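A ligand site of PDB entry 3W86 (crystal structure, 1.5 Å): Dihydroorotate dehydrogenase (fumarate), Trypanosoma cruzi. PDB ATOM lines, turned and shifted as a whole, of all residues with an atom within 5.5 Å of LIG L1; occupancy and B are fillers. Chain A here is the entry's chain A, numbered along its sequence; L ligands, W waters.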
ATOM      1  N   ALA A  19       3.022  20.626 -25.368  1.00  0.00           N
ATOM      2  CA  ALA A  19       1.653  21.078 -25.565  1.00  0.00           C
ATOM      3  C   ALA A  19       0.900  20.023 -26.385  1.00  0.00           C
ATOM      4  O   ALA A  19       1.461  19.382 -27.293  1.00  0.00           O
ATOM      5  CB  ALA A  19       1.666  22.378 -26.348  1.00  0.00           C
ATOM      6  N   ALA A  20      -0.354  19.796 -26.066  1.00  0.00           N
ATOM      7  CA  ALA A  20      -1.118  18.846 -26.844  1.00  0.00           C
ATOM      8  C   ALA A  20      -1.071  19.079 -28.290  1.00  0.00           C
ATOM      9  O   ALA A  20      -1.116  20.232 -28.790  1.00  0.00           O
ATOM     10  CB  ALA A  20      -2.558  18.772 -26.339  1.00  0.00           C
ATOM     11  N   GLY A  21      -0.949  17.984 -29.028  1.00  0.00           N
ATOM     12  CA  GLY A  21      -0.834  18.014 -30.491  1.00  0.00           C
ATOM     13  C   GLY A  21       0.581  17.999 -31.092  1.00  0.00           C
ATOM     14  O   GLY A  21       0.762  17.619 -32.172  1.00  0.00           O
ATOM     15  N   VAL A  22       1.559  18.363 -30.273  1.00  0.00           N
ATOM     16  CA  VAL A  22       2.956  18.396 -30.680  1.00  0.00           C
ATOM     17  C   VAL A  22       3.705  17.197 -30.122  1.00  0.00           C
ATOM     18  O   VAL A  22       3.713  16.991 -28.981  1.00  0.00           O
ATOM     19  CB  VAL A  22       3.623  19.728 -30.294  1.00  0.00           C
ATOM     20  CG1 VAL A  22       5.067  19.719 -30.734  1.00  0.00           C
ATOM     21  CG2 VAL A  22       2.851  20.908 -30.909  1.00  0.00           C
ATOM     22  N   LYS A  44      -2.021  13.632 -28.082  1.00  0.00           N
ATOM     23  CA  LYS A  44      -2.777  14.374 -29.137  1.00  0.00           C
ATOM     24  C   LYS A  44      -4.244  14.340 -28.722  1.00  0.00           C
ATOM     25  O   LYS A  44      -4.777  13.285 -28.384  1.00  0.00           O
ATOM     26  CB  LYS A  44      -2.607  13.713 -30.495  1.00  0.00           C
ATOM     27  CG  LYS A  44      -3.494  14.293 -31.602  1.00  0.00           C
ATOM     28  CD  LYS A  44      -3.274  15.742 -31.959  1.00  0.00           C
ATOM     29  CE  LYS A  44      -4.364  16.256 -32.828  1.00  0.00           C
ATOM     30  NZ  LYS A  44      -4.006  17.674 -33.138  1.00  0.00           N
ATOM     31  N   SER A  45      -4.935  15.438 -28.846  1.00  0.00           N
ATOM     32  CA  SER A  45      -6.394  15.409 -28.559  1.00  0.00           C
ATOM     33  C   SER A  45      -7.052  14.332 -29.464  1.00  0.00           C
ATOM     34  O   SER A  45      -6.798  14.293 -30.652  1.00  0.00           O
ATOM     35  CB  SER A  45      -7.076  16.761 -28.872  1.00  0.00           C
ATOM     36  OG  SER A  45      -6.641  17.729 -27.909  1.00  0.00           O
ATOM     37  N   TYR A  59       0.238  22.786 -41.379  1.00  0.00           N
ATOM     38  CA  TYR A  59       1.110  23.415 -40.383  1.00  0.00           C
ATOM     39  C   TYR A  59       2.210  24.144 -41.067  1.00  0.00           C
ATOM     40  O   TYR A  59       2.834  23.566 -41.950  1.00  0.00           O
ATOM     41  CB  TYR A  59       1.670  22.384 -39.437  1.00  0.00           C
ATOM     42  CG  TYR A  59       2.702  22.948 -38.489  1.00  0.00           C
ATOM     43  CD1 TYR A  59       2.372  23.571 -37.286  1.00  0.00           C
ATOM     44  CD2 TYR A  59       4.027  22.836 -38.786  1.00  0.00           C
ATOM     45  CE1 TYR A  59       3.359  24.108 -36.486  1.00  0.00           C
ATOM     46  CE2 TYR A  59       5.022  23.395 -37.985  1.00  0.00           C
ATOM     47  CZ  TYR A  59       4.686  24.037 -36.842  1.00  0.00           C
ATOM     48  OH  TYR A  59       5.649  24.503 -35.957  1.00  0.00           O
ATOM     49  N   SER A  66       3.937  29.876 -35.493  1.00  0.00           N
ATOM     50  CA  SER A  66       3.337  28.882 -36.383  1.00  0.00           C
ATOM     51  C   SER A  66       1.877  29.176 -36.588  1.00  0.00           C
ATOM     52  O   SER A  66       1.230  29.923 -35.856  1.00  0.00           O
ATOM     53  CB  SER A  66       3.451  27.468 -35.800  1.00  0.00           C
ATOM     54  OG  SER A  66       2.690  27.309 -34.606  1.00  0.00           O
ATOM     55  N   ASN A  68      -1.591  26.697 -37.859  1.00  0.00           N
ATOM     56  CA  ASN A  68      -2.073  25.318 -38.146  1.00  0.00           C
ATOM     57  C   ASN A  68      -3.576  25.220 -38.227  1.00  0.00           C
ATOM     58  O   ASN A  68      -4.338  25.913 -37.562  1.00  0.00           O
ATOM     59  CB  ASN A  68      -1.598  24.309 -37.117  1.00  0.00           C
ATOM     60  CG  ASN A  68      -2.510  24.152 -35.909  1.00  0.00           C
ATOM     61  OD1 ASN A  68      -3.502  23.378 -35.921  1.00  0.00           O
ATOM     62  ND2 ASN A  68      -2.185  24.870 -34.825  1.00  0.00           N
ATOM     63  N   MET A  70      -4.788  21.644 -38.346  1.00  0.00           N
ATOM     64  CA  MET A  70      -4.522  20.249 -38.466  1.00  0.00           C
ATOM     65  C   MET A  70      -5.799  19.493 -38.820  1.00  0.00           C
ATOM     66  O   MET A  70      -5.717  18.478 -39.563  1.00  0.00           O
ATOM     67  CB  MET A  70      -3.883  19.691 -37.225  1.00  0.00           C
ATOM     68  CG  MET A  70      -2.567  20.350 -36.877  1.00  0.00           C
ATOM     69  SD  MET A  70      -1.306  20.340 -38.129  1.00  0.00           S
ATOM     70  CE  MET A  70      -0.803  18.716 -38.020  1.00  0.00           C
ATOM     71  N   LEU A  72      -7.671  17.914 -36.276  1.00  0.00           N
ATOM     72  CA  LEU A  72      -7.814  16.865 -35.331  1.00  0.00           C
ATOM     73  C   LEU A  72      -7.394  15.513 -35.894  1.00  0.00           C
ATOM     74  O   LEU A  72      -8.120  14.495 -35.607  1.00  0.00           O
ATOM     75  CB  LEU A  72      -9.233  16.901 -34.740  1.00  0.00           C
ATOM     76  CG  LEU A  72      -9.591  16.323 -33.432  1.00  0.00           C
ATOM     77  CD1 LEU A  72      -8.567  16.611 -32.300  1.00  0.00           C
ATOM     78  CD2 LEU A  72     -10.954  16.926 -33.008  1.00  0.00           C
ATOM     79  N   SER A  98      -5.424  13.969 -23.689  1.00  0.00           N
ATOM     80  CA  SER A  98      -6.298  15.037 -24.135  1.00  0.00           C
ATOM     81  C   SER A  98      -7.426  14.436 -24.949  1.00  0.00           C
ATOM     82  O   SER A  98      -7.231  13.638 -25.891  1.00  0.00           O
ATOM     83  CB  SER A  98      -5.506  16.013 -24.960  1.00  0.00           C
ATOM     84  OG  SER A  98      -6.388  17.006 -25.471  1.00  0.00           O
ATOM     85  N   GLU A 126      -6.944  15.932 -19.721  1.00  0.00           N
ATOM     86  CA  GLU A 126      -7.025  17.334 -20.220  1.00  0.00           C
ATOM     87  C   GLU A 126      -8.114  17.394 -21.230  1.00  0.00           C
ATOM     88  O   GLU A 126      -8.010  16.876 -22.296  1.00  0.00           O
ATOM     89  CB  GLU A 126      -5.633  17.829 -20.709  1.00  0.00           C
ATOM     90  CG  GLU A 126      -5.676  19.332 -21.095  1.00  0.00           C
ATOM     91  CD  GLU A 126      -4.356  19.879 -21.561  1.00  0.00           C
ATOM     92  OE1 GLU A 126      -4.086  19.738 -22.764  1.00  0.00           O
ATOM     93  OE2 GLU A 126      -3.588  20.491 -20.775  1.00  0.00           O
ATOM     94  N   ASN A 128     -10.172  19.205 -23.936  1.00  0.00           N
ATOM     95  CA  ASN A 128     -10.001  20.325 -24.863  1.00  0.00           C
ATOM     96  C   ASN A 128     -11.356  20.989 -25.204  1.00  0.00           C
ATOM     97  O   ASN A 128     -12.138  20.431 -25.857  1.00  0.00           O
ATOM     98  CB  ASN A 128      -9.295  19.785 -26.103  1.00  0.00           C
ATOM     99  CG  ASN A 128      -8.967  20.841 -27.130  1.00  0.00           C
ATOM    100  OD1 ASN A 128      -9.244  21.937 -26.968  1.00  0.00           O
ATOM    101  ND2 ASN A 128      -8.352  20.415 -28.192  1.00  0.00           N
ATOM    102  N   LYS A 165      -8.439  22.568 -21.261  1.00  0.00           N
ATOM    103  CA  LYS A 165      -7.607  23.373 -22.161  1.00  0.00           C
ATOM    104  C   LYS A 165      -8.476  24.497 -22.772  1.00  0.00           C
ATOM    105  O   LYS A 165      -9.483  24.194 -23.433  1.00  0.00           O
ATOM    106  CB  LYS A 165      -7.013  22.503 -23.234  1.00  0.00           C
ATOM    107  CG  LYS A 165      -6.144  23.229 -24.306  1.00  0.00           C
ATOM    108  CD  LYS A 165      -4.790  23.599 -23.760  1.00  0.00           C
ATOM    109  CE  LYS A 165      -3.901  24.073 -24.894  1.00  0.00           C
ATOM    110  NZ  LYS A 165      -3.402  23.026 -25.758  1.00  0.00           N
ATOM    111  N   VAL A 194      -2.738  28.776 -22.873  1.00  0.00           N
ATOM    112  CA  VAL A 194      -3.812  28.778 -23.802  1.00  0.00           C
ATOM    113  C   VAL A 194      -3.609  27.863 -25.011  1.00  0.00           C
ATOM    114  O   VAL A 194      -2.462  27.458 -25.310  1.00  0.00           O
ATOM    115  CB  VAL A 194      -4.026  30.241 -24.392  1.00  0.00           C
ATOM    116  CG1 VAL A 194      -4.491  31.218 -23.257  1.00  0.00           C
ATOM    117  CG2 VAL A 194      -2.758  30.747 -25.037  1.00  0.00           C
ATOM    118  N   ASN A 195      -4.719  27.514 -25.647  1.00  0.00           N
ATOM    119  CA  ASN A 195      -4.687  27.009 -27.038  1.00  0.00           C
ATOM    120  C   ASN A 195      -4.256  28.116 -28.010  1.00  0.00           C
ATOM    121  O   ASN A 195      -4.009  29.265 -27.596  1.00  0.00           O
ATOM    122  CB  ASN A 195      -6.072  26.412 -27.344  1.00  0.00           C
ATOM    123  CG  ASN A 195      -6.015  25.200 -28.223  1.00  0.00           C
ATOM    124  OD1 ASN A 195      -5.318  25.220 -29.230  1.00  0.00           O
ATOM    125  ND2 ASN A 195      -6.764  24.176 -27.907  1.00  0.00           N
ATOM    126  N   SER A 196      -4.145  27.718 -29.247  1.00  0.00           N
ATOM    127  CA  SER A 196      -3.716  28.683 -30.244  1.00  0.00           C
ATOM    128  C   SER A 196      -4.643  29.857 -30.364  1.00  0.00           C
ATOM    129  O   SER A 196      -5.834  29.765 -30.069  1.00  0.00           O
ATOM    130  CB  SER A 196      -3.468  27.952 -31.564  1.00  0.00           C
ATOM    131  OG  SER A 196      -4.501  27.175 -31.948  1.00  0.00           O
ATOM    132  N   LEU A 221      -2.721  30.366 -34.334  1.00  0.00           N
ATOM    133  CA  LEU A 221      -1.373  30.856 -34.133  1.00  0.00           C
ATOM    134  C   LEU A 221      -0.749  30.392 -32.831  1.00  0.00           C
ATOM    135  O   LEU A 221      -1.335  30.463 -31.756  1.00  0.00           O
ATOM    136  CB  LEU A 221      -1.359  32.344 -34.139  1.00  0.00           C
ATOM    137  CG  LEU A 221      -1.982  33.062 -35.332  1.00  0.00           C
ATOM    138  CD1 LEU A 221      -2.101  34.549 -35.166  1.00  0.00           C
ATOM    139  CD2 LEU A 221      -1.212  32.735 -36.603  1.00  0.00           C
ATOM    140  N   GLY A 222       0.523  30.032 -32.946  1.00  0.00           N
ATOM    141  CA  GLY A 222       1.329  29.736 -31.798  1.00  0.00           C
ATOM    142  C   GLY A 222       2.677  30.383 -31.905  1.00  0.00           C
ATOM    143  O   GLY A 222       3.036  30.961 -32.919  1.00  0.00           O
ATOM    144  N   GLY A 223       3.477  30.325 -30.851  1.00  0.00           N
ATOM    145  CA  GLY A 223       4.808  30.837 -30.834  1.00  0.00           C
ATOM    146  C   GLY A 223       4.987  32.279 -30.325  1.00  0.00           C
ATOM    147  O   GLY A 223       4.178  32.699 -29.459  1.00  0.00           O
ATOM    148  N   ILE A 226       2.232  34.976 -29.606  1.00  0.00           N
ATOM    149  CA  ILE A 226       1.163  34.833 -28.645  1.00  0.00           C
ATOM    150  C   ILE A 226       1.620  34.922 -27.205  1.00  0.00           C
ATOM    151  O   ILE A 226       0.753  34.817 -26.371  1.00  0.00           O
ATOM    152  CB  ILE A 226       0.311  33.525 -28.888  1.00  0.00           C
ATOM    153  CG1 ILE A 226       0.941  32.220 -28.395  1.00  0.00           C
ATOM    154  CG2 ILE A 226      -0.052  33.351 -30.357  1.00  0.00           C
ATOM    155  CD1 ILE A 226      -0.023  31.117 -28.221  1.00  0.00           C
ATOM    156  N   CYS A 249       0.727  27.728 -21.349  1.00  0.00           N
ATOM    157  CA  CYS A 249       1.078  27.299 -22.674  1.00  0.00           C
ATOM    158  C   CYS A 249       1.021  28.533 -23.598  1.00  0.00           C
ATOM    159  O   CYS A 249       0.056  29.141 -23.607  1.00  0.00           O
ATOM    160  CB  CYS A 249       0.032  26.257 -23.133  1.00  0.00           C
ATOM    161  SG  CYS A 249       0.523  25.424 -24.683  1.00  0.00           S
ATOM    162  N   GLY A 250       2.035  28.753 -24.420  1.00  0.00           N
ATOM    163  CA  GLY A 250       2.021  29.788 -25.415  1.00  0.00           C
ATOM    164  C   GLY A 250       3.305  30.560 -25.397  1.00  0.00           C
ATOM    165  O   GLY A 250       3.637  31.180 -24.488  1.00  0.00           O
ATOM    166  N   GLY A 251       4.009  30.457 -26.509  1.00  0.00           N
ATOM    167  CA  GLY A 251       5.166  31.299 -26.681  1.00  0.00           C
ATOM    168  C   GLY A 251       6.391  30.956 -25.947  1.00  0.00           C
ATOM    169  O   GLY A 251       7.321  31.797 -25.866  1.00  0.00           O
ATOM    170  N   VAL A 252       6.500  29.741 -25.385  1.00  0.00           N
ATOM    171  CA  VAL A 252       7.717  29.384 -24.646  1.00  0.00           C
ATOM    172  C   VAL A 252       8.778  28.853 -25.625  1.00  0.00           C
ATOM    173  O   VAL A 252       8.624  27.786 -26.252  1.00  0.00           O
ATOM    174  CB  VAL A 252       7.408  28.293 -23.640  1.00  0.00           C
ATOM    175  CG1 VAL A 252       8.669  27.827 -22.893  1.00  0.00           C
ATOM    176  CG2 VAL A 252       6.416  28.823 -22.634  1.00  0.00           C
ATOM    177  N   GLN A 270       3.844  24.262 -20.775  1.00  0.00           N
ATOM    178  CA  GLN A 270       3.732  23.429 -21.962  1.00  0.00           C
ATOM    179  C   GLN A 270       4.382  24.125 -23.176  1.00  0.00           C
ATOM    180  O   GLN A 270       4.427  25.348 -23.245  1.00  0.00           O
ATOM    181  CB  GLN A 270       2.308  23.122 -22.311  1.00  0.00           C
ATOM    182  CG  GLN A 270       1.417  22.746 -21.143  1.00  0.00           C
ATOM    183  CD  GLN A 270       0.073  22.218 -21.552  1.00  0.00           C
ATOM    184  OE1 GLN A 270      -0.467  22.634 -22.621  1.00  0.00           O
ATOM    185  NE2 GLN A 270      -0.469  21.253 -20.838  1.00  0.00           N
ATOM    186  N   VAL A 271       4.974  23.339 -24.021  1.00  0.00           N
ATOM    187  CA  VAL A 271       5.788  23.833 -25.156  1.00  0.00           C
ATOM    188  C   VAL A 271       5.272  23.214 -26.464  1.00  0.00           C
ATOM    189  O   VAL A 271       5.291  22.002 -26.627  1.00  0.00           O
ATOM    190  CB  VAL A 271       7.277  23.511 -24.967  1.00  0.00           C
ATOM    191  CG1 VAL A 271       8.169  24.212 -26.039  1.00  0.00           C
ATOM    192  CG2 VAL A 271       7.712  23.805 -23.536  1.00  0.00           C
ATOM    193  N   GLY A 272       4.772  24.042 -27.374  1.00  0.00           N
ATOM    194  CA  GLY A 272       4.152  23.631 -28.600  1.00  0.00           C
ATOM    195  C   GLY A 272       5.094  23.946 -29.792  1.00  0.00           C
ATOM    196  O   GLY A 272       5.979  23.143 -30.141  1.00  0.00           O
ATOM    197  N   THR A 273       4.890  25.102 -30.468  1.00  0.00           N
ATOM    198  CA  THR A 273       5.679  25.526 -31.607  1.00  0.00           C
ATOM    199  C   THR A 273       7.152  25.282 -31.369  1.00  0.00           C
ATOM    200  O   THR A 273       7.811  24.735 -32.265  1.00  0.00           O
ATOM    201  CB  THR A 273       5.354  27.006 -31.930  1.00  0.00           C
ATOM    202  OG1 THR A 273       3.952  27.112 -32.189  1.00  0.00           O
ATOM    203  CG2 THR A 273       6.138  27.435 -33.127  1.00  0.00           C
ATOM    204  N   ALA A 274       7.746  25.736 -30.270  1.00  0.00           N
ATOM    205  CA  ALA A 274       9.145  25.662 -30.178  1.00  0.00           C
ATOM    206  C   ALA A 274       9.675  24.188 -30.147  1.00  0.00           C
ATOM    207  O   ALA A 274      10.768  23.935 -30.638  1.00  0.00           O
ATOM    208  CB  ALA A 274       9.683  26.412 -28.972  1.00  0.00           C
ATOM    209  N   GLN A 276       7.957  21.643 -31.653  1.00  0.00           N
ATOM    210  CA  GLN A 276       7.767  21.226 -33.023  1.00  0.00           C
ATOM    211  C   GLN A 276       9.018  21.614 -33.865  1.00  0.00           C
ATOM    212  O   GLN A 276       9.473  20.822 -34.721  1.00  0.00           O
ATOM    213  CB  GLN A 276       6.482  21.773 -33.588  1.00  0.00           C
ATOM    214  CG  GLN A 276       6.246  21.427 -35.070  1.00  0.00           C
ATOM    215  CD  GLN A 276       6.156  19.932 -35.288  1.00  0.00           C
ATOM    216  OE1 GLN A 276       6.568  19.433 -36.364  1.00  0.00           O
ATOM    217  NE2 GLN A 276       5.516  19.276 -34.394  1.00  0.00           N
HETATM  218  N1  LIG L   1      -4.019  21.983 -28.626  1.00  0.00           N
HETATM  219  C1  LIG L   1      -4.800  20.987 -28.138  1.00  0.00           C
HETATM  220  O1  LIG L   1      -5.312  21.154 -27.016  1.00  0.00           O
HETATM  221  N2  LIG L   1      -4.985  19.785 -28.778  1.00  0.00           N
HETATM  222  C2  LIG L   1      -4.468  19.461 -29.939  1.00  0.00           C
HETATM  223  O2  LIG L   1      -4.560  18.323 -30.472  1.00  0.00           O
HETATM  224  C3  LIG L   1      -3.590  20.446 -30.543  1.00  0.00           C
HETATM  225  N3  LIG L   1      -2.953  20.197 -31.650  1.00  0.00           N
HETATM  226  C4  LIG L   1      -1.982  21.052 -32.097  1.00  0.00           C
HETATM  227  C5  LIG L   1      -1.244  20.817 -33.253  1.00  0.00           C
HETATM  228  C6  LIG L   1      -0.249  21.646 -33.701  1.00  0.00           C
HETATM  229  C7  LIG L   1       0.611  21.345 -34.932  1.00  0.00           C
HETATM  230  C8  LIG L   1      -0.004  22.863 -33.019  1.00  0.00           C
HETATM  231  C9  LIG L   1       1.075  23.852 -33.442  1.00  0.00           C
HETATM  232  C10 LIG L   1      -0.736  23.150 -31.905  1.00  0.00           C
HETATM  233  C11 LIG L   1      -1.726  22.302 -31.446  1.00  0.00           C
HETATM  234  N4  LIG L   1      -2.510  22.620 -30.317  1.00  0.00           N
HETATM  235  C12 LIG L   1      -3.389  21.683 -29.781  1.00  0.00           C
HETATM  236  C13 LIG L   1      -2.296  23.859 -29.507  1.00  0.00           C
HETATM  237  C14 LIG L   1      -1.071  23.786 -28.704  1.00  0.00           C
HETATM  238  O3  LIG L   1      -1.269  22.779 -27.673  1.00  0.00           O
HETATM  239  C15 LIG L   1      -0.791  25.080 -27.978  1.00  0.00           C
HETATM  240  O4  LIG L   1      -1.924  25.412 -27.161  1.00  0.00           O
HETATM  241  C16 LIG L   1      -0.502  26.230 -28.961  1.00  0.00           C
HETATM  242  O5  LIG L   1       0.283  25.781 -30.096  1.00  0.00           O
HETATM  243  C17 LIG L   1       0.177  27.401 -28.262  1.00  0.00           C
HETATM  244  O6  LIG L   1       1.437  27.025 -27.692  1.00  0.00           O
HETATM  245  P1  LIG L   1       2.830  27.422 -28.458  1.00  0.00           P
HETATM  246  O7  LIG L   1       3.887  26.778 -27.609  1.00  0.00           O
HETATM  247  O8  LIG L   1       2.909  28.916 -28.532  1.00  0.00           O
HETATM  248  O9  LIG L   1       2.766  26.761 -29.843  1.00  0.00           O
HETATM  249  O1  LG2 L   2      -6.250  21.391 -35.658  1.00  0.00           O
HETATM  250  C1  LG2 L   2      -5.981  20.786 -34.587  1.00  0.00           C
HETATM  251  O2  LG2 L   2      -5.939  19.549 -34.506  1.00  0.00           O
HETATM  252  C2  LG2 L   2      -5.833  21.543 -33.364  1.00  0.00           C
HETATM  253  N1  LG2 L   2      -5.012  22.680 -33.518  1.00  0.00           N
HETATM  254  C3  LG2 L   2      -4.854  23.569 -32.535  1.00  0.00           C
HETATM  255  O3  LG2 L   2      -4.077  24.557 -32.630  1.00  0.00           O
HETATM  256  N2  LG2 L   2      -5.541  23.383 -31.346  1.00  0.00           N
HETATM  257  C4  LG2 L   2      -6.370  22.298 -31.126  1.00  0.00           C
HETATM  258  O4  LG2 L   2      -6.975  22.227 -30.058  1.00  0.00           O
HETATM  259  C5  LG2 L   2      -6.550  21.362 -32.213  1.00  0.00           C
HETATM  260  C6  LG2 L   2      -7.489  20.217 -32.001  1.00  0.00           C
HETATM  261  C7  LG2 L   2      -8.979  20.685 -32.172  1.00  0.00           C
HETATM  262  C8  LG2 L   2      -9.246  20.986 -33.645  1.00  0.00           C
HETATM  263  C9  LG2 L   2     -10.811  21.034 -33.996  1.00  0.00           C
HETATM  264  C10 LG2 L   2     -11.038  20.980 -35.371  1.00  0.00           C
HETATM  265  C11 LG2 L   2     -11.815  19.950 -35.947  1.00  0.00           C
HETATM  266  C12 LG2 L   2     -12.050  19.919 -37.302  1.00  0.00           C
HETATM  267  C13 LG2 L   2     -10.536  21.950 -36.157  1.00  0.00           C
HETATM  268  C14 LG2 L   2     -10.767  21.932 -37.530  1.00  0.00           C
HETATM  269  C15 LG2 L   2     -11.513  20.915 -38.145  1.00  0.00           C
HETATM  270  C16 LG2 L   2     -11.753  20.857 -39.531  1.00  0.00           C
HETATM  271  O5  LG2 L   2     -12.379  19.872 -39.944  1.00  0.00           O
HETATM  272  O6  LG2 L   2     -11.104  21.762 -40.414  1.00  0.00           O
HETATM  273  C17 LG2 L   2     -10.940  23.128 -40.160  1.00  0.00           C
HETATM  274  O   HOH W   1      -0.787  26.915 -32.158  1.00  0.00           O
HETATM  275  O   HOH W   2       4.487  27.459 -25.078  1.00  0.00           O
HETATM  276  O   HOH W   3       6.555  27.317 -28.315  1.00  0.00           O
HETATM  277  O   HOH W   4      -5.928  19.472 -24.792  1.00  0.00           O
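The side-chain amide nitrogen (ND2) of Asn 128 sits at hydrogen-bond distance from the side-chain hydroxyl (OG) of Ser 45 (3.2 Å).
The side-chain amide oxygen (OD1) of Asn 195 sits at hydrogen-bond distance from the side-chain hydroxyl (OG) of Ser 196 (3.4 Å).
The backbone carbonyl oxygen (O) of Val 271 sits at hydrogen-bond distance from the backbone NH (N) of Ala 19, at 2.9 Å.
The side-chain amide oxygen of Asn 68 sits at hydrogen-bond distance from the backbone NH of Met 70 (3.2 Å).
OG1 of Thr 273 lies within hydrogen-bond range of OG of Ser 66, at 2.7 Å.
The side-chain sulfur (SG) of Cys 249 is in hydrogen-bond range of the side-chain amide oxygen (OE1) of Gln 270, 3.6 Å away.
The backbone carbonyl oxygen of Gly 222 lies within hydrogen-bond range of the backbone NH of Ser 66, at 2.9 Å.
N of Val 194 lies within hydrogen-bond range of O of Cys 249, at 2.9 Å.
NZ of Lys 44 sits at hydrogen-bond distance from O2 of LIG L1 (2.8 Å).
The side-chain amide nitrogen (ND2) of Asn 128 sits at hydrogen-bond distance from an oxygen (O1) of LIG L1, at 3.3 Å.
O2 of LG2 L2 sits at hydrogen-bond distance from N of Leu 72 (3.0 Å).
The backbone NH of Thr 273 is in hydrogen-bond range of an oxygen (O9) of LIG L1 (2.8 Å).
An oxygen (O3) of LIG L1 lies within hydrogen-bond range of the side-chain amino group (NZ) of Lys 165 (2.9 Å).
OG of Ser 45 is in hydrogen-bond range of N2 of LIG L1.
O of Ala 20 sits at hydrogen-bond distance from O3 of LIG L1, at 2.8 Å.
The side-chain hydroxyl of Ser 196 sits at hydrogen-bond distance from an oxygen (O3) of LG2 L2 (2.7 Å).
O8 of LIG L1 is in hydrogen-bond range of N of Gly 223 (2.8 Å).
The side-chain amino group (NZ) of Lys 44 is in salt-bridge range of an oxygen (O2) of LG2 L2, at 3.0 Å.
OD1 of Asn 195 sits at hydrogen-bond distance from N2 of LG2 L2 (2.8 Å).
N of Ser 45 sits at hydrogen-bond distance from O2 of LIG L1 (3.3 Å).
O1 of LIG L1 sits at hydrogen-bond distance from ND2 of Asn 195, 3.5 Å away.
An oxygen (O4) of LIG L1 sits at hydrogen-bond distance from the backbone carbonyl oxygen of Val 194 (2.8 Å).
The backbone NH (N) of Met 70 is in hydrogen-bond range of an oxygen (O1) of LG2 L2 (3.1 Å).
The side-chain hydroxyl (OG1) of Thr 273 sits at hydrogen-bond distance from an oxygen (O9) of LIG L1 (2.7 Å).
N of Gly 272 is in hydrogen-bond range of O7 of LIG L1.
The backbone NH (N) of Gly 251 lies within hydrogen-bond range of an oxygen (O8) of LIG L1 (2.8 Å).
The side-chain amide nitrogen (ND2) of Asn 128 sits at hydrogen-bond distance from an oxygen (O4) of LG2 L2 (2.9 Å).
The side-chain sulfur (SG) of Cys 249 is in hydrogen-bond range of an oxygen (O4) of LIG L1 (3.5 Å).
ND2 of Asn 68 lies within hydrogen-bond range of O3 of LG2 L2.
Residues that only touch LIG L1: Ala 19 (3.2 Å), Gly 21 (3.3 Å), Tyr 59 (3.7 Å), Ser 66 (3.99 Å), Asn 68 (3.5 Å), Met 70 (3.9 Å), Ser 196 (3.8 Å), Gly 222 (3.7 Å), Ile 226 (3.7 Å), Gly 250 (3.4 Å) and Val 271 (3.99 Å).
Within 4 Å of LIG L1: Ala 19, Ala 20, Gly 21, Lys 44, Ser 45, Tyr 59, Ser 66, Asn 68, Met 70, Asn 128, Lys 165, Val 194, Asn 195, Ser 196, Gly 222, Gly 223, Ile 226, Cys 249, Gly 250, Gly 251, Val 271, Gly 272 and Thr 273.
N2 of LIG L1 lies close to O4 of LG2 L2 (3.4 Å).
Water W1 lies within hydrogen-bond range of O5 of LIG L1 and N of Gly 222.
Water W3 lies within hydrogen-bond range of the backbone NH of Ala 274 (2.8 Å), an oxygen (O7) of LIG L1 (2.8 Å) and the backbone carbonyl oxygen of Val 252 (3.0 Å).
Water W4 lies within hydrogen-bond range of OG of Ser 98, OE1 of Glu 126 and O1 of LIG L1.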
